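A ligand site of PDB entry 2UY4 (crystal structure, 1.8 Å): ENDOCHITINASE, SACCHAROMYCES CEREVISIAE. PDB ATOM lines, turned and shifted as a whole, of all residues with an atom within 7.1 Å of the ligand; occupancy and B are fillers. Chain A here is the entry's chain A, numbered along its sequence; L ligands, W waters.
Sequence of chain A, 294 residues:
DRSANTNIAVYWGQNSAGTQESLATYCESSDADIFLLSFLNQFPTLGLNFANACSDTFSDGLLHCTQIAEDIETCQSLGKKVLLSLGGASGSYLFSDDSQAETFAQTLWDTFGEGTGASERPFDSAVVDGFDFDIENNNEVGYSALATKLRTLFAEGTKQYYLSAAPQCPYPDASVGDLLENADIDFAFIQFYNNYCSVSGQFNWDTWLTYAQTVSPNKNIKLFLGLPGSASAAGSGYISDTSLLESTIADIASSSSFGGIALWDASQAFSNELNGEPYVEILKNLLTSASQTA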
ATOM      1  N   TYR A  11     -12.713  -4.155 -14.767  1.00  0.00           N
ATOM      2  CA  TYR A  11     -13.527  -3.208 -15.546  1.00  0.00           C
ATOM      3  C   TYR A  11     -14.143  -2.226 -14.548  1.00  0.00           C
ATOM      4  O   TYR A  11     -14.482  -2.629 -13.446  1.00  0.00           O
ATOM      5  CB  TYR A  11     -14.581  -3.952 -16.369  1.00  0.00           C
ATOM      6  CG  TYR A  11     -13.944  -4.574 -17.594  1.00  0.00           C
ATOM      7  CD1 TYR A  11     -13.314  -5.806 -17.530  1.00  0.00           C
ATOM      8  CD2 TYR A  11     -13.952  -3.881 -18.799  1.00  0.00           C
ATOM      9  CE1 TYR A  11     -12.686  -6.350 -18.659  1.00  0.00           C
ATOM     10  CE2 TYR A  11     -13.285  -4.401 -19.934  1.00  0.00           C
ATOM     11  CZ  TYR A  11     -12.660  -5.617 -19.852  1.00  0.00           C
ATOM     12  OH  TYR A  11     -12.022  -6.105 -20.992  1.00  0.00           O
ATOM     13  N   GLN A  14     -19.409   0.947 -15.451  1.00  0.00           N
ATOM     14  CA  GLN A  14     -20.793   0.593 -15.784  1.00  0.00           C
ATOM     15  C   GLN A  14     -21.662   0.262 -14.567  1.00  0.00           C
ATOM     16  O   GLN A  14     -22.860  -0.010 -14.708  1.00  0.00           O
ATOM     17  CB  GLN A  14     -20.826  -0.546 -16.833  1.00  0.00           C
ATOM     18  CG  GLN A  14     -20.354  -0.050 -18.223  1.00  0.00           C
ATOM     19  CD  GLN A  14     -21.269   1.052 -18.774  1.00  0.00           C
ATOM     20  OE1 GLN A  14     -22.465   0.836 -19.007  1.00  0.00           O
ATOM     21  NE2 GLN A  14     -20.712   2.254 -18.942  1.00  0.00           N
ATOM     22  N   SER A  16     -22.082  -2.271 -12.421  1.00  0.00           N
ATOM     23  CA  SER A  16     -22.836  -3.523 -12.409  1.00  0.00           C
ATOM     24  C   SER A  16     -23.544  -3.699 -11.053  1.00  0.00           C
ATOM     25  O   SER A  16     -24.718  -4.106 -11.011  1.00  0.00           O
ATOM     26  CB  SER A  16     -21.896  -4.691 -12.694  1.00  0.00           C
ATOM     27  OG  SER A  16     -22.554  -5.926 -12.489  1.00  0.00           O
ATOM     28  N   SER A  38     -14.993   1.712 -18.735  1.00  0.00           N
ATOM     29  CA  SER A  38     -16.070   1.098 -19.521  1.00  0.00           C
ATOM     30  C   SER A  38     -17.232   2.085 -19.590  1.00  0.00           C
ATOM     31  O   SER A  38     -17.894   2.297 -18.559  1.00  0.00           O
ATOM     32  CB  SER A  38     -16.547  -0.160 -18.812  1.00  0.00           C
ATOM     33  OG  SER A  38     -15.435  -1.010 -18.577  1.00  0.00           O
ATOM     34  N   PHE A  39     -17.501   2.703 -20.753  1.00  0.00           N
ATOM     35  CA  PHE A  39     -16.907   2.397 -22.056  1.00  0.00           C
ATOM     36  C   PHE A  39     -16.926   3.616 -22.969  1.00  0.00           C
ATOM     37  O   PHE A  39     -17.772   4.482 -22.792  1.00  0.00           O
ATOM     38  CB  PHE A  39     -17.787   1.384 -22.797  1.00  0.00           C
ATOM     39  CG  PHE A  39     -17.754  -0.001 -22.238  1.00  0.00           C
ATOM     40  CD1 PHE A  39     -16.619  -0.790 -22.361  1.00  0.00           C
ATOM     41  CD2 PHE A  39     -18.911  -0.540 -21.647  1.00  0.00           C
ATOM     42  CE1 PHE A  39     -16.606  -2.106 -21.866  1.00  0.00           C
ATOM     43  CE2 PHE A  39     -18.913  -1.839 -21.155  1.00  0.00           C
ATOM     44  CZ  PHE A  39     -17.763  -2.631 -21.271  1.00  0.00           C
ATOM     45  N   SER A  85     -11.660   1.332 -22.421  1.00  0.00           N
ATOM     46  CA  SER A  85     -12.285   0.184 -23.102  1.00  0.00           C
ATOM     47  C   SER A  85     -13.316   0.665 -24.132  1.00  0.00           C
ATOM     48  O   SER A  85     -14.279   1.403 -23.800  1.00  0.00           O
ATOM     49  CB  SER A  85     -12.961  -0.803 -22.125  1.00  0.00           C
ATOM     50  OG  SER A  85     -13.327  -1.991 -22.823  1.00  0.00           O
ATOM     51  N   GLY A  87     -16.336  -0.157 -26.788  1.00  0.00           N
ATOM     52  CA  GLY A  87     -17.372  -1.093 -27.189  1.00  0.00           C
ATOM     53  C   GLY A  87     -18.333  -1.404 -26.101  1.00  0.00           C
ATOM     54  O   GLY A  87     -19.093  -0.557 -25.672  1.00  0.00           O
ATOM     55  N   GLY A  88     -18.225  -2.637 -25.595  1.00  0.00           N
ATOM     56  CA  GLY A  88     -19.113  -3.143 -24.579  1.00  0.00           C
ATOM     57  C   GLY A  88     -20.286  -3.836 -25.221  1.00  0.00           C
ATOM     58  O   GLY A  88     -20.651  -3.581 -26.390  1.00  0.00           O
ATOM     59  N   ALA A  89     -20.927  -4.711 -24.452  1.00  0.00           N
ATOM     60  CA  ALA A  89     -22.182  -5.323 -24.896  1.00  0.00           C
ATOM     61  C   ALA A  89     -23.155  -4.177 -25.192  1.00  0.00           C
ATOM     62  O   ALA A  89     -23.090  -3.160 -24.516  1.00  0.00           O
ATOM     63  CB  ALA A  89     -22.741  -6.236 -23.803  1.00  0.00           C
ATOM     64  N   SER A  90     -24.018  -4.287 -26.183  1.00  0.00           N
ATOM     65  CA  SER A  90     -24.906  -3.139 -26.491  1.00  0.00           C
ATOM     66  C   SER A  90     -24.056  -1.880 -26.779  1.00  0.00           C
ATOM     67  O   SER A  90     -22.851  -1.970 -26.907  1.00  0.00           O
ATOM     68  CB  SER A  90     -25.897  -2.866 -25.352  1.00  0.00           C
ATOM     69  OG  SER A  90     -25.235  -2.325 -24.204  1.00  0.00           O
ATOM     70  N   ASP A 132      -8.572  -0.879 -24.583  1.00  0.00           N
ATOM     71  CA  ASP A 132      -9.038  -2.266 -24.537  1.00  0.00           C
ATOM     72  C   ASP A 132     -10.131  -2.387 -25.581  1.00  0.00           C
ATOM     73  O   ASP A 132     -11.019  -1.524 -25.663  1.00  0.00           O
ATOM     74  CB  ASP A 132      -9.666  -2.554 -23.167  1.00  0.00           C
ATOM     75  CG  ASP A 132     -10.314  -3.956 -23.083  1.00  0.00           C
ATOM     76  OD1 ASP A 132      -9.631  -4.968 -23.402  1.00  0.00           O
ATOM     77  OD2 ASP A 132     -11.503  -4.041 -22.662  1.00  0.00           O
ATOM     78  N   ASP A 134     -13.219  -4.177 -26.330  1.00  0.00           N
ATOM     79  CA  ASP A 134     -14.239  -5.088 -25.804  1.00  0.00           C
ATOM     80  C   ASP A 134     -15.378  -5.043 -26.845  1.00  0.00           C
ATOM     81  O   ASP A 134     -16.466  -4.559 -26.590  1.00  0.00           O
ATOM     82  CB  ASP A 134     -14.684  -4.666 -24.397  1.00  0.00           C
ATOM     83  CG  ASP A 134     -15.794  -5.561 -23.866  1.00  0.00           C
ATOM     84  OD1 ASP A 134     -15.970  -6.667 -24.409  1.00  0.00           O
ATOM     85  OD2 ASP A 134     -16.491  -5.141 -22.907  1.00  0.00           O
ATOM     86  N   GLU A 136     -18.262  -6.468 -28.993  1.00  0.00           N
ATOM     87  CA  GLU A 136     -19.242  -7.541 -28.750  1.00  0.00           C
ATOM     88  C   GLU A 136     -20.382  -7.619 -29.785  1.00  0.00           C
ATOM     89  O   GLU A 136     -21.416  -8.236 -29.508  1.00  0.00           O
ATOM     90  CB  GLU A 136     -19.745  -7.446 -27.287  1.00  0.00           C
ATOM     91  CG  GLU A 136     -18.570  -7.432 -26.246  1.00  0.00           C
ATOM     92  CD  GLU A 136     -18.883  -7.933 -24.836  1.00  0.00           C
ATOM     93  OE1 GLU A 136     -20.051  -8.247 -24.531  1.00  0.00           O
ATOM     94  OE2 GLU A 136     -17.946  -7.989 -23.994  1.00  0.00           O
ATOM     95  N   ALA A 166     -10.880  -8.127 -25.333  1.00  0.00           N
ATOM     96  CA  ALA A 166     -11.746  -8.822 -24.419  1.00  0.00           C
ATOM     97  C   ALA A 166     -12.636  -9.871 -25.100  1.00  0.00           C
ATOM     98  O   ALA A 166     -13.873  -9.767 -25.051  1.00  0.00           O
ATOM     99  CB  ALA A 166     -12.598  -7.802 -23.607  1.00  0.00           C
ATOM    100  N   PRO A 167     -12.017 -10.904 -25.708  1.00  0.00           N
ATOM    101  CA  PRO A 167     -12.810 -11.967 -26.339  1.00  0.00           C
ATOM    102  C   PRO A 167     -13.640 -12.715 -25.303  1.00  0.00           C
ATOM    103  O   PRO A 167     -13.253 -12.773 -24.140  1.00  0.00           O
ATOM    104  CB  PRO A 167     -11.732 -12.952 -26.830  1.00  0.00           C
ATOM    105  CG  PRO A 167     -10.557 -12.745 -25.843  1.00  0.00           C
ATOM    106  CD  PRO A 167     -10.573 -11.214 -25.748  1.00  0.00           C
ATOM    107  N   PHE A 189      -8.003 -10.243 -22.154  1.00  0.00           N
ATOM    108  CA  PHE A 189      -8.885 -10.488 -21.026  1.00  0.00           C
ATOM    109  C   PHE A 189     -10.023 -11.392 -21.485  1.00  0.00           C
ATOM    110  O   PHE A 189     -11.059 -10.920 -21.950  1.00  0.00           O
ATOM    111  CB  PHE A 189      -9.404  -9.141 -20.483  1.00  0.00           C
ATOM    112  CG  PHE A 189      -8.308  -8.153 -20.149  1.00  0.00           C
ATOM    113  CD1 PHE A 189      -7.317  -8.471 -19.214  1.00  0.00           C
ATOM    114  CD2 PHE A 189      -8.276  -6.884 -20.747  1.00  0.00           C
ATOM    115  CE1 PHE A 189      -6.305  -7.533 -18.901  1.00  0.00           C
ATOM    116  CE2 PHE A 189      -7.285  -5.980 -20.443  1.00  0.00           C
ATOM    117  CZ  PHE A 189      -6.315  -6.297 -19.548  1.00  0.00           C
ATOM    118  N   GLN A 191     -13.197 -13.671 -21.437  1.00  0.00           N
ATOM    119  CA  GLN A 191     -14.390 -13.823 -20.602  1.00  0.00           C
ATOM    120  C   GLN A 191     -14.783 -15.278 -20.478  1.00  0.00           C
ATOM    121  O   GLN A 191     -15.399 -15.846 -21.389  1.00  0.00           O
ATOM    122  CB  GLN A 191     -15.560 -12.990 -21.179  1.00  0.00           C
ATOM    123  CG  GLN A 191     -15.139 -11.608 -21.604  1.00  0.00           C
ATOM    124  CD  GLN A 191     -16.281 -10.800 -22.155  1.00  0.00           C
ATOM    125  OE1 GLN A 191     -17.416 -10.927 -21.686  1.00  0.00           O
ATOM    126  NE2 GLN A 191     -15.992  -9.925 -23.100  1.00  0.00           N
ATOM    127  N   TYR A 193     -17.148 -16.612 -18.895  1.00  0.00           N
ATOM    128  CA  TYR A 193     -18.472 -16.499 -18.303  1.00  0.00           C
ATOM    129  C   TYR A 193     -19.483 -16.226 -19.424  1.00  0.00           C
ATOM    130  O   TYR A 193     -19.090 -15.829 -20.533  1.00  0.00           O
ATOM    131  CB  TYR A 193     -18.497 -15.421 -17.185  1.00  0.00           C
ATOM    132  CG  TYR A 193     -17.960 -14.038 -17.538  1.00  0.00           C
ATOM    133  CD1 TYR A 193     -16.608 -13.715 -17.345  1.00  0.00           C
ATOM    134  CD2 TYR A 193     -18.821 -13.021 -18.007  1.00  0.00           C
ATOM    135  CE1 TYR A 193     -16.121 -12.431 -17.648  1.00  0.00           C
ATOM    136  CE2 TYR A 193     -18.324 -11.723 -18.310  1.00  0.00           C
ATOM    137  CZ  TYR A 193     -16.986 -11.445 -18.135  1.00  0.00           C
ATOM    138  OH  TYR A 193     -16.465 -10.190 -18.425  1.00  0.00           O
ATOM    139  N   ASN A 194     -20.768 -16.459 -19.125  1.00  0.00           N
ATOM    140  CA  ASN A 194     -21.845 -16.380 -20.101  1.00  0.00           C
ATOM    141  C   ASN A 194     -21.627 -17.325 -21.312  1.00  0.00           C
ATOM    142  O   ASN A 194     -22.117 -17.040 -22.408  1.00  0.00           O
ATOM    143  CB  ASN A 194     -22.081 -14.930 -20.572  1.00  0.00           C
ATOM    144  CG  ASN A 194     -22.573 -13.995 -19.456  1.00  0.00           C
ATOM    145  OD1 ASN A 194     -23.347 -14.378 -18.579  1.00  0.00           O
ATOM    146  ND2 ASN A 194     -22.130 -12.736 -19.520  1.00  0.00           N
ATOM    147  N   ALA A 233     -23.071 -10.495 -11.235  1.00  0.00           N
ATOM    148  CA  ALA A 233     -22.333  -9.785 -12.284  1.00  0.00           C
ATOM    149  C   ALA A 233     -22.503 -10.357 -13.699  1.00  0.00           C
ATOM    150  O   ALA A 233     -22.257  -9.651 -14.693  1.00  0.00           O
ATOM    151  CB  ALA A 233     -20.880  -9.699 -11.921  1.00  0.00           C
ATOM    152  N   ALA A 234     -22.917 -11.617 -13.779  1.00  0.00           N
ATOM    153  CA  ALA A 234     -23.172 -12.290 -15.056  1.00  0.00           C
ATOM    154  C   ALA A 234     -24.225 -13.404 -14.880  1.00  0.00           C
ATOM    155  O   ALA A 234     -24.512 -13.834 -13.750  1.00  0.00           O
ATOM    156  CB  ALA A 234     -21.852 -12.837 -15.655  1.00  0.00           C
ATOM    157  N   LEU A 263     -11.738  -9.000 -14.003  1.00  0.00           N
ATOM    158  CA  LEU A 263     -13.063  -9.078 -13.382  1.00  0.00           C
ATOM    159  C   LEU A 263     -14.054  -8.119 -13.970  1.00  0.00           C
ATOM    160  O   LEU A 263     -13.773  -6.949 -14.087  1.00  0.00           O
ATOM    161  CB  LEU A 263     -12.958  -8.821 -11.879  1.00  0.00           C
ATOM    162  CG  LEU A 263     -12.156  -9.937 -11.175  1.00  0.00           C
ATOM    163  CD1 LEU A 263     -11.425  -9.407  -9.940  1.00  0.00           C
ATOM    164  CD2 LEU A 263     -13.059 -11.122 -10.880  1.00  0.00           C
ATOM    165  N   TRP A 264     -15.263  -8.627 -14.247  1.00  0.00           N
ATOM    166  CA  TRP A 264     -16.373  -7.763 -14.563  1.00  0.00           C
ATOM    167  C   TRP A 264     -17.304  -7.712 -13.354  1.00  0.00           C
ATOM    168  O   TRP A 264     -17.961  -8.703 -13.074  1.00  0.00           O
ATOM    169  CB  TRP A 264     -17.197  -8.317 -15.744  1.00  0.00           C
ATOM    170  CG  TRP A 264     -18.355  -7.410 -15.965  1.00  0.00           C
ATOM    171  CD1 TRP A 264     -19.636  -7.567 -15.502  1.00  0.00           C
ATOM    172  CD2 TRP A 264     -18.334  -6.159 -16.658  1.00  0.00           C
ATOM    173  NE1 TRP A 264     -20.409  -6.477 -15.890  1.00  0.00           N
ATOM    174  CE2 TRP A 264     -19.636  -5.612 -16.601  1.00  0.00           C
ATOM    175  CE3 TRP A 264     -17.330  -5.460 -17.366  1.00  0.00           C
ATOM    176  CZ2 TRP A 264     -19.979  -4.391 -17.218  1.00  0.00           C
ATOM    177  CZ3 TRP A 264     -17.667  -4.231 -17.967  1.00  0.00           C
ATOM    178  CH2 TRP A 264     -18.982  -3.723 -17.882  1.00  0.00           C
HETATM  179  C1  LIG L   1     -21.403  -5.972 -20.103  1.00  0.00           C
HETATM  180  C2  LIG L   1     -19.150  -6.204 -20.821  1.00  0.00           C
HETATM  181  C3  LIG L   1     -17.174  -7.412 -20.400  1.00  0.00           C
HETATM  182  C4  LIG L   1     -15.734  -7.487 -20.820  1.00  0.00           C
HETATM  183  N1  LIG L   1     -23.926  -6.843 -20.446  1.00  0.00           N
HETATM  184  N2  LIG L   1     -19.862  -5.236 -21.436  1.00  0.00           N
HETATM  185  N3  LIG L   1     -21.056  -5.112 -21.052  1.00  0.00           N
HETATM  186  N4  LIG L   1     -17.867  -6.491 -21.035  1.00  0.00           N
HETATM  187  O1  LIG L   1     -23.477  -4.683 -19.117  1.00  0.00           O
HETATM  188  O2  LIG L   1     -22.847  -6.823 -18.105  1.00  0.00           O
HETATM  189  O3  LIG L   1     -17.612  -8.179 -19.535  1.00  0.00           O
HETATM  190  S1  LIG L   1     -22.949  -6.069 -19.388  1.00  0.00           S
HETATM  191  S2  LIG L   1     -20.104  -6.965 -19.677  1.00  0.00           S
HETATM  192  O   HOH W   1     -23.092  -6.916 -14.796  1.00  0.00           O
HETATM  193  O   HOH W   2     -23.344  -1.826 -19.640  1.00  0.00           O
HETATM  194  O   HOH W   3     -22.254  -2.701 -22.075  1.00  0.00           O
HETATM  195  O   HOH W   4     -12.764  -9.153 -20.675  1.00  0.00           O
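OH of Tyr 193 sits at hydrogen-bond distance from O3 of the ligand (2.6 Å).
OD2 of Asp 134 lies within hydrogen-bond range of N4 of the ligand (2.7 Å).
A nitrogen (N2) of the ligand lies within hydrogen-bond range of the backbone NH of Ala 89, 3.2 Å away.
NE1 of Trp 264 sits at hydrogen-bond distance from O2 of the ligand, 3.3 Å away.
The side-chain carboxylate (OE2) of Glu 136 sits at hydrogen-bond distance from a nitrogen (N4) of the ligand (3.3 Å).
OE1 of Gln 191 sits close to O3 of the ligand (3.5 Å).
OH of Tyr 193 sits at hydrogen-bond distance from OE1 of Gln 191 (3.5 Å).
The side-chain carboxylate (OD1) of Asp 134 lies close to the side-chain carboxylate (OE2) of Glu 136 (2.4 Å).
The backbone carbonyl oxygen (O) of Asp 134 sits at hydrogen-bond distance from the backbone NH (N) of Gly 88 (2.8 Å).
The side-chain amide nitrogen (NE2) of Gln 191 sits at hydrogen-bond distance from the side-chain carboxylate (OE2) of Glu 136, 2.9 Å away.
O of Ala 166 sits at hydrogen-bond distance from NE2 of Gln 191 (2.9 Å).
The backbone carbonyl oxygen (O) of Pro 167 lies within hydrogen-bond range of the backbone NH (N) of Gln 191, 2.8 Å away.
The side-chain carboxylate of Asp 132 lies within hydrogen-bond range of the side-chain hydroxyl of Tyr 11.
N of Tyr 11 is in hydrogen-bond range of O of Leu 263 (3.1 Å).
Residues that only touch the ligand: Phe 39 (3.3 Å), Tyr 11 (3.7 Å) and Gly 88 (3.8 Å).
Hydrophobic or aromatic side chains that line the ligand: Tyr 11, Phe 39, Ala 89, Tyr 193 and Trp 264.
Within 4 Å of the ligand: Tyr 11, Phe 39, Gly 88, Ala 89, Asp 134, Glu 136, Gln 191, Tyr 193 and Trp 264.
The nearest printed residue that does not touch the ligand is Ala 166 (4.2 Å).
Water W3 lies within hydrogen-bond range of the backbone carbonyl oxygen of Ala 89 (2.6 Å) and a nitrogen (N3) of the ligand (2.9 Å).
Water W2 lies within hydrogen-bond range of the side-chain amide oxygen (OE1) of Gln 14 (2.9 Å) and an oxygen (O1) of the ligand (2.9 Å).
Water W1 lies within hydrogen-bond range of OG of Ser 16 (2.6 Å), O of Ala 233 (2.9 Å), NE1 of Trp 264 (2.9 Å) and O2 of the ligand (3.3 Å).
Water W4 bridges the backbone carbonyl oxygen (O) of Phe 189 and the side-chain hydroxyl (OH) of Tyr 11.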
